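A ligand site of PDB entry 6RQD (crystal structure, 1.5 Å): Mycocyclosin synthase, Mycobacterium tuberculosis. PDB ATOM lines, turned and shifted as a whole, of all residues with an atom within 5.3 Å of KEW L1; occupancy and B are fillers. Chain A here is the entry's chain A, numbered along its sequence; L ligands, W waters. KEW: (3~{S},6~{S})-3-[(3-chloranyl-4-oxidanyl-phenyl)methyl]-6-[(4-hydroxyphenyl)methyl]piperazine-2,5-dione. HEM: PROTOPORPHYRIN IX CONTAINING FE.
Water W4 lies within hydrogen-bond range of an oxygen (O01) of KEW L1 (2.5 Å), the side-chain amide oxygen of Gln 385 (2.7 Å) and the guanidinium group of Arg 386 (2.8 Å).
Water W1 lies within hydrogen-bond range of O of Thr 77 (2.7 Å) and O16 of KEW L1 (2.9 Å).
OG of Ser 237 lies within hydrogen-bond range of NH2 of Arg 386, at 2.8 Å.
O of Ala 167 lies within hydrogen-bond range of OG1 of Thr 77.
O of Phe 168 sits at hydrogen-bond distance from N of Gln 385, at 2.7 Å.
The side-chain amide nitrogen (ND2) of Asn 85 lies within hydrogen-bond range of the side-chain hydroxyl (OG1) of Thr 229, 2.9 Å away.
A nitrogen (N20) of KEW L1 sits at hydrogen-bond distance from an oxygen (O2D) of HEM L2, at 3.3 Å.
Merely in contact with KEW L1: Met 62 (3.5 Å), Val 78 (3.5 Å), Val 82 (3.7 Å), Val 83 (3.4 Å), Ala 167 (3.6 Å), Phe 168 (3.5 Å), Thr 229 (3.7 Å) and Gln 385 (3.7 Å).
Hydrophobic or aromatic side chains within 4 Å of KEW L1: Met 62, Val 78, Val 83, Ala 167 and Phe 168.
The nearest printed residue that does not touch KEW L1 is Ala 233 (4.1 Å).
The side-chain amide nitrogen (ND2) of Asn 85 is in hydrogen-bond range of an oxygen (O21) of KEW L1, 3.1 Å away.
The guanidinium group (NH2) of Arg 386 lies within hydrogen-bond range of an oxygen (O01) of KEW L1 (3.4 Å).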
ATOM      1  N   MET A  62      20.789  15.727  26.094  1.00  0.00           N
ATOM      2  CA  MET A  62      20.095  16.935  25.632  1.00  0.00           C
ATOM      3  C   MET A  62      19.974  16.918  24.117  1.00  0.00           C
ATOM      4  O   MET A  62      18.887  17.149  23.562  1.00  0.00           O
ATOM      5  CB  MET A  62      20.815  18.209  26.102  1.00  0.00           C
ATOM      6  CG  MET A  62      20.380  19.495  25.348  1.00  0.00           C
ATOM      7  SD  MET A  62      21.209  21.022  25.849  1.00  0.00           S
ATOM      8  CE  MET A  62      20.654  21.071  27.542  1.00  0.00           C
ATOM      9  N   THR A  77      11.791  26.033  19.224  1.00  0.00           N
ATOM     10  CA  THR A  77      11.765  27.432  18.789  1.00  0.00           C
ATOM     11  C   THR A  77      13.069  27.851  18.112  1.00  0.00           C
ATOM     12  O   THR A  77      13.234  29.018  17.752  1.00  0.00           O
ATOM     13  CB  THR A  77      11.462  28.367  19.956  1.00  0.00           C
ATOM     14  OG1 THR A  77      12.569  28.358  20.877  1.00  0.00           O
ATOM     15  CG2 THR A  77      10.185  27.925  20.669  1.00  0.00           C
ATOM     16  N   VAL A  78      13.987  26.906  17.918  1.00  0.00           N
ATOM     17  CA  VAL A  78      15.257  27.127  17.231  1.00  0.00           C
ATOM     18  C   VAL A  78      15.490  25.965  16.279  1.00  0.00           C
ATOM     19  O   VAL A  78      14.824  24.935  16.379  1.00  0.00           O
ATOM     20  CB  VAL A  78      16.416  27.206  18.231  1.00  0.00           C
ATOM     21  CG1 VAL A  78      16.241  28.386  19.191  1.00  0.00           C
ATOM     22  CG2 VAL A  78      16.520  25.907  19.037  1.00  0.00           C
ATOM     23  N   VAL A  82      20.715  23.695  16.899  1.00  0.00           N
ATOM     24  CA  VAL A  82      20.989  24.631  17.997  1.00  0.00           C
ATOM     25  C   VAL A  82      20.740  24.021  19.363  1.00  0.00           C
ATOM     26  O   VAL A  82      21.292  24.506  20.352  1.00  0.00           O
ATOM     27  CB  VAL A  82      20.191  25.925  17.727  1.00  0.00           C
ATOM     28  CG1 VAL A  82      20.419  26.959  18.806  1.00  0.00           C
ATOM     29  CG2 VAL A  82      20.561  26.495  16.343  1.00  0.00           C
ATOM     30  N   VAL A  83      19.945  22.960  19.474  1.00  0.00           N
ATOM     31  CA  VAL A  83      19.849  22.259  20.753  1.00  0.00           C
ATOM     32  C   VAL A  83      21.234  21.777  21.213  1.00  0.00           C
ATOM     33  O   VAL A  83      21.491  21.681  22.419  1.00  0.00           O
ATOM     34  CB  VAL A  83      18.836  21.100  20.644  1.00  0.00           C
ATOM     35  CG1 VAL A  83      18.804  20.292  21.933  1.00  0.00           C
ATOM     36  CG2 VAL A  83      17.459  21.657  20.330  1.00  0.00           C
ATOM     37  N   ASN A  85      23.997  23.426  20.878  1.00  0.00           N
ATOM     38  CA  ASN A  85      24.782  24.655  20.771  1.00  0.00           C
ATOM     39  C   ASN A  85      26.141  24.512  21.420  1.00  0.00           C
ATOM     40  O   ASN A  85      27.164  24.852  20.807  1.00  0.00           O
ATOM     41  CB  ASN A  85      23.969  25.764  21.417  1.00  0.00           C
ATOM     42  CG  ASN A  85      24.449  27.139  21.029  1.00  0.00           C
ATOM     43  OD1 ASN A  85      24.925  27.361  19.912  1.00  0.00           O
ATOM     44  ND2 ASN A  85      24.308  28.086  21.950  1.00  0.00           N
ATOM     45  N   ALA A 167      10.423  33.666  21.679  1.00  0.00           N
ATOM     46  CA  ALA A 167      11.519  32.719  21.545  1.00  0.00           C
ATOM     47  C   ALA A 167      11.539  31.700  22.677  1.00  0.00           C
ATOM     48  O   ALA A 167      11.957  30.545  22.494  1.00  0.00           O
ATOM     49  CB  ALA A 167      12.836  33.488  21.543  1.00  0.00           C
ATOM     50  N   PHE A 168      11.160  32.119  23.883  1.00  0.00           N
ATOM     51  CA  PHE A 168      11.187  31.243  25.051  1.00  0.00           C
ATOM     52  C   PHE A 168       9.809  30.728  25.428  1.00  0.00           C
ATOM     53  O   PHE A 168       9.617  30.273  26.553  1.00  0.00           O
ATOM     54  CB  PHE A 168      11.955  31.912  26.193  1.00  0.00           C
ATOM     55  CG  PHE A 168      13.437  31.899  25.952  1.00  0.00           C
ATOM     56  CD1 PHE A 168      14.184  30.800  26.308  1.00  0.00           C
ATOM     57  CD2 PHE A 168      14.055  32.943  25.285  1.00  0.00           C
ATOM     58  CE1 PHE A 168      15.536  30.758  26.048  1.00  0.00           C
ATOM     59  CE2 PHE A 168      15.398  32.899  25.021  1.00  0.00           C
ATOM     60  CZ  PHE A 168      16.145  31.805  25.401  1.00  0.00           C
ATOM     61  N   TRP A 182      13.922  34.779  14.773  1.00  0.00           N
ATOM     62  CA  TRP A 182      15.208  34.094  14.714  1.00  0.00           C
ATOM     63  C   TRP A 182      15.995  34.507  13.480  1.00  0.00           C
ATOM     64  O   TRP A 182      17.163  34.918  13.574  1.00  0.00           O
ATOM     65  CB  TRP A 182      14.999  32.582  14.730  1.00  0.00           C
ATOM     66  CG  TRP A 182      16.281  31.817  14.632  1.00  0.00           C
ATOM     67  CD1 TRP A 182      16.853  31.286  13.509  1.00  0.00           C
ATOM     68  CD2 TRP A 182      17.175  31.507  15.706  1.00  0.00           C
ATOM     69  NE1 TRP A 182      18.029  30.652  13.824  1.00  0.00           N
ATOM     70  CE2 TRP A 182      18.252  30.783  15.159  1.00  0.00           C
ATOM     71  CE3 TRP A 182      17.159  31.771  17.083  1.00  0.00           C
ATOM     72  CZ2 TRP A 182      19.314  30.333  15.954  1.00  0.00           C
ATOM     73  CZ3 TRP A 182      18.208  31.318  17.857  1.00  0.00           C
ATOM     74  CH2 TRP A 182      19.272  30.598  17.284  1.00  0.00           C
ATOM     75  N   VAL A 228      23.177  35.177  19.065  1.00  0.00           N
ATOM     76  CA  VAL A 228      21.740  35.175  19.318  1.00  0.00           C
ATOM     77  C   VAL A 228      21.413  34.358  20.566  1.00  0.00           C
ATOM     78  O   VAL A 228      20.628  34.804  21.419  1.00  0.00           O
ATOM     79  CB  VAL A 228      20.953  34.669  18.093  1.00  0.00           C
ATOM     80  CG1 VAL A 228      19.459  34.598  18.406  1.00  0.00           C
ATOM     81  CG2 VAL A 228      21.207  35.569  16.904  1.00  0.00           C
ATOM     82  N   THR A 229      21.996  33.166  20.675  1.00  0.00           N
ATOM     83  CA  THR A 229      21.666  32.282  21.788  1.00  0.00           C
ATOM     84  C   THR A 229      22.189  32.809  23.124  1.00  0.00           C
ATOM     85  O   THR A 229      21.516  32.682  24.153  1.00  0.00           O
ATOM     86  CB  THR A 229      22.168  30.853  21.531  1.00  0.00           C
ATOM     87  OG1 THR A 229      23.595  30.860  21.381  1.00  0.00           O
ATOM     88  CG2 THR A 229      21.529  30.257  20.287  1.00  0.00           C
ATOM     89  N   GLY A 232      19.998  35.718  24.154  1.00  0.00           N
ATOM     90  CA  GLY A 232      18.669  35.252  24.511  1.00  0.00           C
ATOM     91  C   GLY A 232      18.592  34.495  25.816  1.00  0.00           C
ATOM     92  O   GLY A 232      17.798  34.852  26.703  1.00  0.00           O
ATOM     93  N   ALA A 233      19.388  33.428  25.938  1.00  0.00           N
ATOM     94  CA  ALA A 233      19.428  32.649  27.166  1.00  0.00           C
ATOM     95  C   ALA A 233      19.890  33.495  28.342  1.00  0.00           C
ATOM     96  O   ALA A 233      19.320  33.414  29.444  1.00  0.00           O
ATOM     97  CB  ALA A 233      20.343  31.434  26.967  1.00  0.00           C
ATOM     98  N   SER A 237      17.247  34.482  31.284  1.00  0.00           N
ATOM     99  CA  SER A 237      17.562  33.775  32.521  1.00  0.00           C
ATOM    100  C   SER A 237      17.854  34.753  33.656  1.00  0.00           C
ATOM    101  O   SER A 237      17.329  34.597  34.760  1.00  0.00           O
ATOM    102  CB  SER A 237      18.722  32.802  32.305  1.00  0.00           C
ATOM    103  OG  SER A 237      18.314  31.776  31.418  1.00  0.00           O
ATOM    104  N   PHE A 280      12.512  28.398  36.307  1.00  0.00           N
ATOM    105  CA  PHE A 280      12.354  27.433  35.220  1.00  0.00           C
ATOM    106  C   PHE A 280      10.974  26.794  35.308  1.00  0.00           C
ATOM    107  O   PHE A 280      10.646  26.121  36.301  1.00  0.00           O
ATOM    108  CB  PHE A 280      13.442  26.363  35.205  1.00  0.00           C
ATOM    109  CG  PHE A 280      14.675  26.763  34.440  1.00  0.00           C
ATOM    110  CD1 PHE A 280      15.469  27.802  34.885  1.00  0.00           C
ATOM    111  CD2 PHE A 280      15.038  26.104  33.268  1.00  0.00           C
ATOM    112  CE1 PHE A 280      16.604  28.195  34.175  1.00  0.00           C
ATOM    113  CE2 PHE A 280      16.186  26.478  32.567  1.00  0.00           C
ATOM    114  CZ  PHE A 280      16.971  27.528  33.026  1.00  0.00           C
ATOM    115  N   GLN A 385       8.877  29.237  28.984  1.00  0.00           N
ATOM    116  CA  GLN A 385       9.961  28.441  29.549  1.00  0.00           C
ATOM    117  C   GLN A 385      10.439  28.961  30.891  1.00  0.00           C
ATOM    118  O   GLN A 385      11.173  28.261  31.581  1.00  0.00           O
ATOM    119  CB  GLN A 385      11.132  28.318  28.568  1.00  0.00           C
ATOM    120  CG  GLN A 385      10.776  27.558  27.307  1.00  0.00           C
ATOM    121  CD  GLN A 385      11.925  27.472  26.325  1.00  0.00           C
ATOM    122  OE1 GLN A 385      13.084  27.328  26.716  1.00  0.00           O
ATOM    123  NE2 GLN A 385      11.611  27.568  25.038  1.00  0.00           N
ATOM    124  N   ARG A 386      10.028  30.181  31.255  1.00  0.00           N
ATOM    125  CA  ARG A 386      10.287  30.746  32.576  1.00  0.00           C
ATOM    126  C   ARG A 386       8.954  31.091  33.223  1.00  0.00           C
ATOM    127  O   ARG A 386       7.939  31.301  32.560  1.00  0.00           O
ATOM    128  CB  ARG A 386      11.130  32.032  32.476  1.00  0.00           C
ATOM    129  CG  ARG A 386      12.533  31.817  31.944  1.00  0.00           C
ATOM    130  CD  ARG A 386      13.367  30.877  32.829  1.00  0.00           C
ATOM    131  NE  ARG A 386      14.716  30.749  32.279  1.00  0.00           N
ATOM    132  CZ  ARG A 386      15.049  29.885  31.317  1.00  0.00           C
ATOM    133  NH1 ARG A 386      14.141  29.073  30.807  1.00  0.00           N
ATOM    134  NH2 ARG A 386      16.294  29.849  30.870  1.00  0.00           N
HETATM  135  C02 KEW L   1      17.216  27.105  27.513  1.00  0.00           C
HETATM  136  C03 KEW L   1      16.695  26.236  26.586  1.00  0.00           C
HETATM  137  C04 KEW L   1      17.447  25.325  26.046  1.00  0.00           C
HETATM  138  C05 KEW L   1      18.793  25.273  26.373  1.00  0.00           C
HETATM  139  C06 KEW L   1      19.659  24.205  25.730  1.00  0.00           C
HETATM  140  C07 KEW L   1      20.161  24.516  24.305  1.00  0.00           C
HETATM  141  C08 KEW L   1      19.077  25.047  23.305  1.00  0.00           C
HETATM  142  C10 KEW L   1      19.968  27.314  23.371  1.00  0.00           C
HETATM  143  C11 KEW L   1      19.289  28.392  24.270  1.00  0.00           C
HETATM  144  C12 KEW L   1      18.344  29.226  23.495  1.00  0.00           C
HETATM  145  C13 KEW L   1      17.097  28.801  23.189  1.00  0.00           C
HETATM  146  C14 KEW L   1      16.206  29.578  22.437  1.00  0.00           C
HETATM  147  C15 KEW L   1      16.644  30.779  21.957  1.00  0.00           C
HETATM  148  C17 KEW L   1      17.891  31.218  22.280  1.00  0.00           C
HETATM  149  C18 KEW L   1      18.714  30.449  23.026  1.00  0.00           C
HETATM  150  C19 KEW L   1      21.211  26.706  23.979  1.00  0.00           C
HETATM  151  C23 KEW L   1      19.265  26.130  27.320  1.00  0.00           C
HETATM  152  C24 KEW L   1      18.414  27.050  27.903  1.00  0.00           C
HETATM  153  N09 KEW L   1      19.075  26.346  22.921  1.00  0.00           N
HETATM  154  N20 KEW L   1      21.275  25.456  24.394  1.00  0.00           N
HETATM  155  O01 KEW L   1      16.450  27.981  28.057  1.00  0.00           O
HETATM  156  O16 KEW L   1      15.820  31.546  21.241  1.00  0.00           O
HETATM  157  O21 KEW L   1      22.197  27.405  24.101  1.00  0.00           O
HETATM  158  O22 KEW L   1      18.200  24.353  22.880  1.00  0.00           O
HETATM  159 CL1  KEW L   1      18.842  28.216  29.051  1.00  0.00          CL
HETATM  160  CHA HEM L   2      22.189  26.540  30.611  1.00  0.00           C
HETATM  161  CHB HEM L   2      20.128  28.525  34.420  1.00  0.00           C
HETATM  162  CHC HEM L   2      22.351  32.726  33.345  1.00  0.00           C
HETATM  163  CHD HEM L   2      23.598  30.895  29.090  1.00  0.00           C
HETATM  164  C1A HEM L   2      21.522  26.705  31.787  1.00  0.00           C
HETATM  165  C2A HEM L   2      20.895  25.641  32.493  1.00  0.00           C
HETATM  166  C3A HEM L   2      20.305  26.221  33.566  1.00  0.00           C
HETATM  167  C4A HEM L   2      20.560  27.610  33.505  1.00  0.00           C
HETATM  168  CMA HEM L   2      19.517  25.505  34.622  1.00  0.00           C
HETATM  169  CAA HEM L   2      20.950  24.168  32.151  1.00  0.00           C
HETATM  170  CBA HEM L   2      19.893  23.713  31.140  1.00  0.00           C
HETATM  171  CGA HEM L   2      19.894  22.222  30.920  1.00  0.00           C
HETATM  172  O1A HEM L   2      20.767  21.556  31.489  1.00  0.00           O
HETATM  173  O2A HEM L   2      19.015  21.738  30.244  1.00  0.00           O
HETATM  174  C1B HEM L   2      20.549  29.874  34.454  1.00  0.00           C
HETATM  175  C2B HEM L   2      20.158  30.791  35.436  1.00  0.00           C
HETATM  176  C3B HEM L   2      20.778  31.961  35.141  1.00  0.00           C
HETATM  177  C4B HEM L   2      21.553  31.746  33.933  1.00  0.00           C
HETATM  178  CMB HEM L   2      19.258  30.532  36.606  1.00  0.00           C
HETATM  179  CAB HEM L   2      20.742  33.246  35.811  1.00  0.00           C
HETATM  180  CBB HEM L   2      20.727  33.396  37.107  1.00  0.00           C
HETATM  181  C1C HEM L   2      22.937  32.620  32.100  1.00  0.00           C
HETATM  182  C2C HEM L   2      23.704  33.580  31.437  1.00  0.00           C
HETATM  183  C3C HEM L   2      24.035  32.994  30.230  1.00  0.00           C
HETATM  184  C4C HEM L   2      23.461  31.721  30.181  1.00  0.00           C
HETATM  185  CMC HEM L   2      24.065  34.928  31.989  1.00  0.00           C
HETATM  186  CAC HEM L   2      24.820  33.546  29.143  1.00  0.00           C
HETATM  187  CBC HEM L   2      25.341  34.740  29.220  1.00  0.00           C
HETATM  188  C1D HEM L   2      23.256  29.565  29.178  1.00  0.00           C
HETATM  189  C2D HEM L   2      23.488  28.654  28.059  1.00  0.00           C
HETATM  190  C3D HEM L   2      23.082  27.452  28.489  1.00  0.00           C
HETATM  191  C4D HEM L   2      22.624  27.615  29.872  1.00  0.00           C
HETATM  192  CMD HEM L   2      24.007  29.034  26.706  1.00  0.00           C
HETATM  193  CAD HEM L   2      23.065  26.164  27.702  1.00  0.00           C
HETATM  194  CBD HEM L   2      24.261  25.332  28.041  1.00  0.00           C
HETATM  195  CGD HEM L   2      24.248  24.116  27.215  1.00  0.00           C
HETATM  196  O1D HEM L   2      25.061  23.233  27.459  1.00  0.00           O
HETATM  197  O2D HEM L   2      23.444  23.904  26.334  1.00  0.00           O
HETATM  198  NA  HEM L   2      21.304  27.870  32.418  1.00  0.00           N
HETATM  199  NB  HEM L   2      21.342  30.486  33.638  1.00  0.00           N
HETATM  200  NC  HEM L   2      22.842  31.536  31.346  1.00  0.00           N
HETATM  201  ND  HEM L   2      22.875  28.871  30.210  1.00  0.00           N
HETATM  202 FE   HEM L   2      22.255  29.614  31.962  1.00  0.00          FE
HETATM  203  O   HOH W   1      13.768  31.203  19.228  1.00  0.00           O
HETATM  204  O   HOH W   2      15.448  24.599  22.602  1.00  0.00           O
HETATM  205  O   HOH W   3      20.171  30.004  30.710  1.00  0.00           O
HETATM  206  O   HOH W   4      14.422  26.914  28.984  1.00  0.00           O
HETATM  207  O   HOH W   5      16.410  34.233  20.629  1.00  0.00           O
